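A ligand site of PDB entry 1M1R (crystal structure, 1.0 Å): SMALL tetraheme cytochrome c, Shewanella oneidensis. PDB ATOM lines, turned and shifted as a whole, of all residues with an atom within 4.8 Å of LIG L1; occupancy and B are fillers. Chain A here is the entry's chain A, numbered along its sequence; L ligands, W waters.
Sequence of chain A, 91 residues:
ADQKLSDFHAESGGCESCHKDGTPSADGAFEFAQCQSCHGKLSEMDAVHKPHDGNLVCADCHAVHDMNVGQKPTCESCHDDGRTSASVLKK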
ATOM      1  N   SER A   6      11.152 -16.790  -8.779  1.00  0.00           N
ATOM      2  CA  SER A   6      11.127 -16.898  -7.318  1.00  0.00           C
ATOM      3  C   SER A   6      11.776 -18.161  -6.838  1.00  0.00           C
ATOM      4  O   SER A   6      12.596 -18.198  -5.911  1.00  0.00           O
ATOM      5  CB  SER A   6       9.716 -16.761  -6.805  1.00  0.00           C
ATOM      6  OG  SER A   6       8.898 -17.728  -7.468  1.00  0.00           O
ATOM      7  N   ASP A   7      11.449 -19.280  -7.522  1.00  0.00           N
ATOM      8  CA  ASP A   7      11.982 -20.578  -7.166  1.00  0.00           C
ATOM      9  C   ASP A   7      13.430 -20.715  -7.384  1.00  0.00           C
ATOM     10  O   ASP A   7      14.193 -21.282  -6.604  1.00  0.00           O
ATOM     11  CB  ASP A   7      11.159 -21.688  -7.848  1.00  0.00           C
ATOM     12  CG  ASP A   7       9.717 -21.747  -7.417  1.00  0.00           C
ATOM     13  OD1 ASP A   7       9.535 -21.691  -6.207  1.00  0.00           O
ATOM     14  OD2 ASP A   7       8.937 -21.796  -8.291  1.00  0.00           O
ATOM     15  N   HIS A   9      15.647 -18.212  -7.248  1.00  0.00           N
ATOM     16  CA  HIS A   9      16.295 -17.531  -6.156  1.00  0.00           C
ATOM     17  C   HIS A   9      16.222 -18.303  -4.846  1.00  0.00           C
ATOM     18  O   HIS A   9      17.181 -18.307  -4.061  1.00  0.00           O
ATOM     19  CB  HIS A   9      15.726 -16.134  -6.010  1.00  0.00           C
ATOM     20  CG  HIS A   9      16.072 -15.109  -7.023  1.00  0.00           C
ATOM     21  ND1 HIS A   9      15.399 -14.961  -8.221  1.00  0.00           N
ATOM     22  CD2 HIS A   9      16.975 -14.130  -7.023  1.00  0.00           C
ATOM     23  CE1 HIS A   9      15.940 -13.919  -8.887  1.00  0.00           C
ATOM     24  NE2 HIS A   9      16.890 -13.378  -8.170  1.00  0.00           N
ATOM     25  N   ALA A  10      15.070 -18.878  -4.560  1.00  0.00           N
ATOM     26  CA  ALA A  10      14.921 -19.601  -3.308  1.00  0.00           C
ATOM     27  C   ALA A  10      15.881 -20.783  -3.198  1.00  0.00           C
ATOM     28  O   ALA A  10      16.246 -21.172  -2.094  1.00  0.00           O
ATOM     29  CB  ALA A  10      13.469 -20.061  -3.117  1.00  0.00           C
ATOM     30  N   GLY A  14      16.761 -19.499   0.040  1.00  0.00           N
ATOM     31  CA  GLY A  14      15.448 -19.708   0.653  1.00  0.00           C
ATOM     32  C   GLY A  14      14.463 -18.611   0.270  1.00  0.00           C
ATOM     33  O   GLY A  14      14.802 -17.599  -0.349  1.00  0.00           O
ATOM     34  N   CYS A  15      13.224 -18.772   0.732  1.00  0.00           N
ATOM     35  CA  CYS A  15      12.221 -17.725   0.576  1.00  0.00           C
ATOM     36  C   CYS A  15      12.676 -16.457   1.307  1.00  0.00           C
ATOM     37  O   CYS A  15      12.349 -15.344   0.913  1.00  0.00           O
ATOM     38  CB  CYS A  15      10.881 -18.154   1.151  1.00  0.00           C
ATOM     39  SG  CYS A  15      10.244 -19.724   0.465  1.00  0.00           S
ATOM     40  N   SER A  17      15.487 -15.139   1.217  1.00  0.00           N
ATOM     41  CA  SER A  17      16.383 -14.308   0.406  1.00  0.00           C
ATOM     42  C   SER A  17      15.695 -13.001   0.068  1.00  0.00           C
ATOM     43  O   SER A  17      16.365 -11.966  -0.099  1.00  0.00           O
ATOM     44  CB  SER A  17      16.705 -15.029  -0.903  1.00  0.00           C
ATOM     45  OG  SER A  17      17.815 -14.413  -1.563  1.00  0.00           O
ATOM     46  N   CYS A  18      14.365 -13.062  -0.093  1.00  0.00           N
ATOM     47  CA  CYS A  18      13.613 -11.842  -0.462  1.00  0.00           C
ATOM     48  C   CYS A  18      12.592 -11.441   0.618  1.00  0.00           C
ATOM     49  O   CYS A  18      12.222 -10.248   0.613  1.00  0.00           O
ATOM     50  CB  CYS A  18      12.863 -12.071  -1.745  1.00  0.00           C
ATOM     51  SG  CYS A  18      14.000 -12.300  -3.118  1.00  0.00           S
ATOM     52  N   HIS A  19      12.053 -12.378   1.432  1.00  0.00           N
ATOM     53  CA  HIS A  19      10.980 -12.116   2.327  1.00  0.00           C
ATOM     54  C   HIS A  19      11.373 -12.326   3.766  1.00  0.00           C
ATOM     55  O   HIS A  19      11.978 -13.363   4.099  1.00  0.00           O
ATOM     56  CB  HIS A  19       9.839 -13.083   2.091  1.00  0.00           C
ATOM     57  CG  HIS A  19       9.172 -12.991   0.759  1.00  0.00           C
ATOM     58  ND1 HIS A  19       8.575 -11.856   0.262  1.00  0.00           N
ATOM     59  CD2 HIS A  19       8.973 -13.979  -0.185  1.00  0.00           C
ATOM     60  CE1 HIS A  19       8.048 -12.158  -0.897  1.00  0.00           C
ATOM     61  NE2 HIS A  19       8.274 -13.420  -1.249  1.00  0.00           N
ATOM     62  N   GLY A  22      10.521 -15.547   5.408  1.00  0.00           N
ATOM     63  CA  GLY A  22       9.897 -16.226   4.280  1.00  0.00           C
ATOM     64  C   GLY A  22       8.459 -15.845   4.003  1.00  0.00           C
ATOM     65  O   GLY A  22       7.797 -16.496   3.226  1.00  0.00           O
ATOM     66  N   PRO A  24       5.647 -12.770   2.830  1.00  0.00           N
ATOM     67  CA  PRO A  24       5.617 -11.491   2.090  1.00  0.00           C
ATOM     68  C   PRO A  24       5.098 -10.353   2.935  1.00  0.00           C
ATOM     69  O   PRO A  24       4.205 -10.507   3.771  1.00  0.00           O
ATOM     70  CB  PRO A  24       4.640 -11.789   0.971  1.00  0.00           C
ATOM     71  CG  PRO A  24       3.728 -12.827   1.511  1.00  0.00           C
ATOM     72  CD  PRO A  24       4.641 -13.726   2.303  1.00  0.00           C
ATOM     73  N   SER A  25       5.653  -9.174   2.697  1.00  0.00           N
ATOM     74  CA  SER A  25       5.173  -7.931   3.242  1.00  0.00           C
ATOM     75  C   SER A  25       3.971  -7.488   2.442  1.00  0.00           C
ATOM     76  O   SER A  25       3.711  -7.859   1.326  1.00  0.00           O
ATOM     77  CB  SER A  25       6.188  -6.807   3.163  1.00  0.00           C
ATOM     78  OG  SER A  25       6.417  -6.317   1.880  1.00  0.00           O
ATOM     79  N   ALA A  26       3.211  -6.542   3.055  1.00  0.00           N
ATOM     80  CA  ALA A  26       2.076  -5.960   2.337  1.00  0.00           C
ATOM     81  C   ALA A  26       2.548  -4.958   1.301  1.00  0.00           C
ATOM     82  O   ALA A  26       1.930  -4.835   0.267  1.00  0.00           O
ATOM     83  CB  ALA A  26       1.224  -5.270   3.366  1.00  0.00           C
ATOM     84  N   ASP A  27       3.528  -4.165   1.627  1.00  0.00           N
ATOM     85  CA  ASP A  27       4.028  -2.954   0.931  1.00  0.00           C
ATOM     86  C   ASP A  27       4.983  -3.299  -0.250  1.00  0.00           C
ATOM     87  O   ASP A  27       5.105  -2.473  -1.169  1.00  0.00           O
ATOM     88  CB  ASP A  27       4.715  -2.008   1.936  1.00  0.00           C
ATOM     89  CG  ASP A  27       3.962  -1.237   2.989  1.00  0.00           C
ATOM     90  OD1 ASP A  27       2.719  -1.264   2.954  1.00  0.00           O
ATOM     91  OD2 ASP A  27       4.574  -0.533   3.880  1.00  0.00           O
ATOM     92  N   GLY A  28       5.703  -4.376  -0.189  1.00  0.00           N
ATOM     93  CA  GLY A  28       6.764  -4.744  -1.094  1.00  0.00           C
ATOM     94  C   GLY A  28       8.070  -3.973  -0.876  1.00  0.00           C
ATOM     95  O   GLY A  28       9.040  -4.197  -1.627  1.00  0.00           O
ATOM     96  N   GLU A  31      11.043  -6.325   0.175  1.00  0.00           N
ATOM     97  CA  GLU A  31      11.472  -7.163  -0.968  1.00  0.00           C
ATOM     98  C   GLU A  31      12.289  -6.286  -1.963  1.00  0.00           C
ATOM     99  O   GLU A  31      13.289  -6.778  -2.475  1.00  0.00           O
ATOM    100  CB  GLU A  31      10.197  -7.710  -1.660  1.00  0.00           C
ATOM    101  CG  GLU A  31       9.535  -8.829  -0.832  1.00  0.00           C
ATOM    102  CD  GLU A  31       8.670  -8.390   0.335  1.00  0.00           C
ATOM    103  OE1 GLU A  31       8.403  -7.174   0.506  1.00  0.00           O
ATOM    104  OE2 GLU A  31       8.233  -9.283   1.108  1.00  0.00           O
ATOM    105  N   ALA A  59       9.505  -5.270  -8.790  1.00  0.00           N
ATOM    106  CA  ALA A  59       8.329  -6.095  -8.900  1.00  0.00           C
ATOM    107  C   ALA A  59       7.235  -5.479  -9.729  1.00  0.00           C
ATOM    108  O   ALA A  59       6.260  -6.159 -10.143  1.00  0.00           O
ATOM    109  CB  ALA A  59       7.770  -6.461  -7.523  1.00  0.00           C
ATOM    110  N   VAL A  64       8.093 -12.123 -10.104  1.00  0.00           N
ATOM    111  CA  VAL A  64       9.029 -13.225 -10.006  1.00  0.00           C
ATOM    112  C   VAL A  64       8.379 -14.519  -9.731  1.00  0.00           C
ATOM    113  O   VAL A  64       8.968 -15.570 -10.101  1.00  0.00           O
ATOM    114  CB  VAL A  64      10.164 -12.973  -8.972  1.00  0.00           C
ATOM    115  CG1 VAL A  64      10.989 -11.749  -9.391  1.00  0.00           C
ATOM    116  CG2 VAL A  64       9.612 -12.776  -7.563  1.00  0.00           C
ATOM    117  N   HIS A  65       7.150 -14.549  -9.199  1.00  0.00           N
ATOM    118  CA  HIS A  65       6.473 -15.812  -8.995  1.00  0.00           C
ATOM    119  C   HIS A  65       5.717 -16.334 -10.243  1.00  0.00           C
ATOM    120  O   HIS A  65       5.395 -17.502 -10.303  1.00  0.00           O
ATOM    121  CB  HIS A  65       5.405 -15.667  -7.857  1.00  0.00           C
ATOM    122  CG  HIS A  65       6.060 -15.673  -6.477  1.00  0.00           C
ATOM    123  ND1 HIS A  65       6.239 -16.814  -5.788  1.00  0.00           N
ATOM    124  CD2 HIS A  65       6.567 -14.736  -5.701  1.00  0.00           C
ATOM    125  CE1 HIS A  65       6.836 -16.540  -4.639  1.00  0.00           C
ATOM    126  NE2 HIS A  65       7.089 -15.270  -4.529  1.00  0.00           N
HETATM  127 FE1  LIG L   1       7.695 -14.340  -2.899  1.00  0.00          FE
HETATM  128  C1  LIG L   1       5.090 -12.220  -3.341  1.00  0.00           C
HETATM  129  C2  LIG L   1       5.749 -16.437  -1.079  1.00  0.00           C
HETATM  130  C3  LIG L   1      10.258 -16.573  -2.662  1.00  0.00           C
HETATM  131  C4  LIG L   1       9.777 -12.064  -4.267  1.00  0.00           C
HETATM  132  N1  LIG L   1       5.801 -14.331  -2.324  1.00  0.00           N
HETATM  133  C5  LIG L   1       4.825 -13.398  -2.716  1.00  0.00           C
HETATM  134  C6  LIG L   1       3.561 -13.793  -2.162  1.00  0.00           C
HETATM  135  C7  LIG L   1       3.779 -14.934  -1.431  1.00  0.00           C
HETATM  136  C8  LIG L   1       5.170 -15.251  -1.596  1.00  0.00           C
HETATM  137  C9  LIG L   1       2.755 -15.750  -0.717  1.00  0.00           C
HETATM  138  C10 LIG L   1       2.243 -13.042  -2.339  1.00  0.00           C
HETATM  139  C11 LIG L   1       1.920 -12.041  -1.368  1.00  0.00           C
HETATM  140  C12 LIG L   1       0.563 -11.471  -1.538  1.00  0.00           C
HETATM  141  O1  LIG L   1       0.068 -10.832  -0.589  1.00  0.00           O
HETATM  142  O2  LIG L   1      -0.275 -11.884  -2.434  1.00  0.00           O
HETATM  143  N2  LIG L   1       7.977 -16.103  -2.032  1.00  0.00           N
HETATM  144  C13 LIG L   1       7.008 -16.837  -1.323  1.00  0.00           C
HETATM  145  C14 LIG L   1       7.566 -18.140  -0.914  1.00  0.00           C
HETATM  146  C15 LIG L   1       8.834 -18.201  -1.339  1.00  0.00           C
HETATM  147  C16 LIG L   1       9.074 -16.927  -2.082  1.00  0.00           C
HETATM  148  C17 LIG L   1       6.792 -19.158  -0.135  1.00  0.00           C
HETATM  149  C18 LIG L   1       9.820 -19.301  -1.233  1.00  0.00           C
HETATM  150  C19 LIG L   1       9.452 -20.569  -1.937  1.00  0.00           C
HETATM  151  N3  LIG L   1       9.606 -14.326  -3.428  1.00  0.00           N
HETATM  152  C20 LIG L   1      10.531 -15.321  -3.260  1.00  0.00           C
HETATM  153  C21 LIG L   1      11.864 -14.902  -3.623  1.00  0.00           C
HETATM  154  C22 LIG L   1      11.738 -13.611  -4.041  1.00  0.00           C
HETATM  155  C23 LIG L   1      10.338 -13.286  -3.906  1.00  0.00           C
HETATM  156  C24 LIG L   1      13.100 -15.741  -3.430  1.00  0.00           C
HETATM  157  C25 LIG L   1      12.804 -12.669  -4.440  1.00  0.00           C
HETATM  158  C26 LIG L   1      13.548 -13.065  -5.711  1.00  0.00           C
HETATM  159  N4  LIG L   1       7.431 -12.546  -3.704  1.00  0.00           N
HETATM  160  C27 LIG L   1       8.460 -11.643  -4.133  1.00  0.00           C
HETATM  161  C28 LIG L   1       7.912 -10.352  -4.401  1.00  0.00           C
HETATM  162  C29 LIG L   1       6.587 -10.347  -4.092  1.00  0.00           C
HETATM  163  C30 LIG L   1       6.314 -11.773  -3.738  1.00  0.00           C
HETATM  164  C31 LIG L   1       8.684  -9.117  -4.958  1.00  0.00           C
HETATM  165  C32 LIG L   1       5.614  -9.230  -4.202  1.00  0.00           C
HETATM  166  C33 LIG L   1       5.811  -8.150  -3.175  1.00  0.00           C
HETATM  167  C34 LIG L   1       5.532  -8.497  -1.662  1.00  0.00           C
HETATM  168  O3  LIG L   1       5.991  -9.593  -1.395  1.00  0.00           O
HETATM  169  O4  LIG L   1       5.221  -7.720  -0.962  1.00  0.00           O
HETATM  170 FE1  LG2 L   2      17.932 -11.726  -8.615  1.00  0.00          FE
HETATM  171  C1  LG2 L   2      19.050 -13.461 -11.319  1.00  0.00           C
HETATM  172  C2  LG2 L   2      15.557 -10.274 -10.536  1.00  0.00           C
HETATM  173  C3  LG2 L   2      16.426 -10.563  -5.836  1.00  0.00           C
HETATM  174  C4  LG2 L   2      20.653 -12.605  -6.845  1.00  0.00           C
HETATM  175  N1  LG2 L   2      17.402 -11.834 -10.547  1.00  0.00           N
HETATM  176  C5  LG2 L   2      17.958 -12.639 -11.488  1.00  0.00           C
HETATM  177  C6  LG2 L   2      17.283 -12.422 -12.797  1.00  0.00           C
HETATM  178  C7  LG2 L   2      16.331 -11.492 -12.577  1.00  0.00           C
HETATM  179  C8  LG2 L   2      16.415 -11.124 -11.151  1.00  0.00           C
HETATM  180  C9  LG2 L   2      15.430 -10.844 -13.575  1.00  0.00           C
HETATM  181  C10 LG2 L   2      17.650 -13.089 -14.058  1.00  0.00           C
HETATM  182  C11 LG2 L   2      18.651 -12.305 -14.891  1.00  0.00           C
HETATM  183  C12 LG2 L   2      19.049 -13.032 -16.131  1.00  0.00           C
HETATM  184  O1  LG2 L   2      20.061 -13.811 -16.069  1.00  0.00           O
HETATM  185  O2  LG2 L   2      18.422 -12.902 -17.194  1.00  0.00           O
HETATM  186  N2  LG2 L   2      16.351 -10.644  -8.236  1.00  0.00           N
HETATM  187  C13 LG2 L   2      15.511 -10.028  -9.177  1.00  0.00           C
HETATM  188  C14 LG2 L   2      14.468  -9.292  -8.507  1.00  0.00           C
HETATM  189  C15 LG2 L   2      14.635  -9.459  -7.151  1.00  0.00           C
HETATM  190  C16 LG2 L   2      15.835 -10.280  -7.048  1.00  0.00           C
HETATM  191  C17 LG2 L   2      13.351  -8.571  -9.231  1.00  0.00           C
HETATM  192  C18 LG2 L   2      13.769  -9.038  -6.084  1.00  0.00           C
HETATM  193  C19 LG2 L   2      12.315  -9.411  -6.187  1.00  0.00           C
HETATM  194  N3  LG2 L   2      18.452 -11.593  -6.715  1.00  0.00           N
HETATM  195  C20 LG2 L   2      17.675 -11.157  -5.693  1.00  0.00           C
HETATM  196  C21 LG2 L   2      18.397 -11.264  -4.396  1.00  0.00           C
HETATM  197  C22 LG2 L   2      19.632 -11.766  -4.705  1.00  0.00           C
HETATM  198  C23 LG2 L   2      19.656 -11.976  -6.157  1.00  0.00           C
HETATM  199  C24 LG2 L   2      17.850 -10.913  -3.064  1.00  0.00           C
HETATM  200  C25 LG2 L   2      20.799 -11.925  -3.817  1.00  0.00           C
HETATM  201  C26 LG2 L   2      20.622 -12.776  -2.598  1.00  0.00           C
HETATM  202  N4  LG2 L   2      19.492 -12.827  -9.003  1.00  0.00           N
HETATM  203  C27 LG2 L   2      20.582 -13.066  -8.129  1.00  0.00           C
HETATM  204  C28 LG2 L   2      21.548 -13.929  -8.816  1.00  0.00           C
HETATM  205  C29 LG2 L   2      21.071 -14.187 -10.058  1.00  0.00           C
HETATM  206  C30 LG2 L   2      19.816 -13.503 -10.174  1.00  0.00           C
HETATM  207  C31 LG2 L   2      22.857 -14.311  -8.175  1.00  0.00           C
HETATM  208  C32 LG2 L   2      21.729 -15.039 -11.078  1.00  0.00           C
HETATM  209  C33 LG2 L   2      22.634 -14.234 -12.064  1.00  0.00           C
HETATM  210  C34 LG2 L   2      21.861 -13.662 -13.252  1.00  0.00           C
HETATM  211  O3  LG2 L   2      21.203 -14.517 -13.935  1.00  0.00           O
HETATM  212  O4  LG2 L   2      21.915 -12.434 -13.456  1.00  0.00           O
HETATM  213  O   HOH W   1      -0.281 -12.998  -5.025  1.00  0.00           O
HETATM  214  O   HOH W   2      -2.673 -10.734  -1.379  1.00  0.00           O
HETATM  215  O   HOH W   3       7.904  -9.963  -8.160  1.00  0.00           O
HETATM  216  O   HOH W   4       1.502  -8.706  -0.204  1.00  0.00           O
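An oxygen (O4) of LIG L1 sits close to the backbone NH of Gly 28 (3.5 Å). An iron atom (FE1) of LIG L1 is bound by a ring nitrogen (NE2) of His 65, 2.0 Å away. The side-chain hydroxyl (OG) of Ser 25 is in hydrogen-bond range of an oxygen (O4) of LIG L1 (3.4 Å). O of Ser 25 sits close to O4 of LIG L1. The side-chain sulfur (SG) of Cys 18 is covalently linked to a carbon (C25) of LIG L1, 1.8 Å away. NE2 of His 19 is bound to FE1 of LIG L1 (2.0 Å). C18 of LIG L1 is bonded to SG of Cys 15 (1.8 Å). An iron atom (FE1) of LG2 L2 is bound by a ring nitrogen (NE2) of His 9 (2.0 Å).
The side-chain carboxylate of Glu 31 sits at hydrogen-bond distance from the side-chain hydroxyl of Ser 25 (2.6 Å). ND1 of His 19 lies within hydrogen-bond range of OE2 of Glu 31 (2.7 Å). The backbone NH (N) of Gly 28 lies within hydrogen-bond range of the side-chain hydroxyl (OG) of Ser 25 (2.9 Å). The backbone NH (N) of Ser 6 lies within hydrogen-bond range of the backbone carbonyl oxygen (O) of Val 64 (2.8 Å). ND1 of His 65 is in hydrogen-bond range of OG of Ser 6 (3.3 Å).
The side-chain carboxylate (OE2) of Glu 31 sits close to an oxygen (O3) of LIG L1, 3.4 Å away. Merely in contact with LIG L1: Ser 6, His 9, Ala 10, Gly 14, Pro 24, Ala 59 and Val 64. Of the 19 residues printed, 14 come within 4 Å of LIG L1.
Water W4 bridges O1 of LIG L1 and O of Ser 25.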
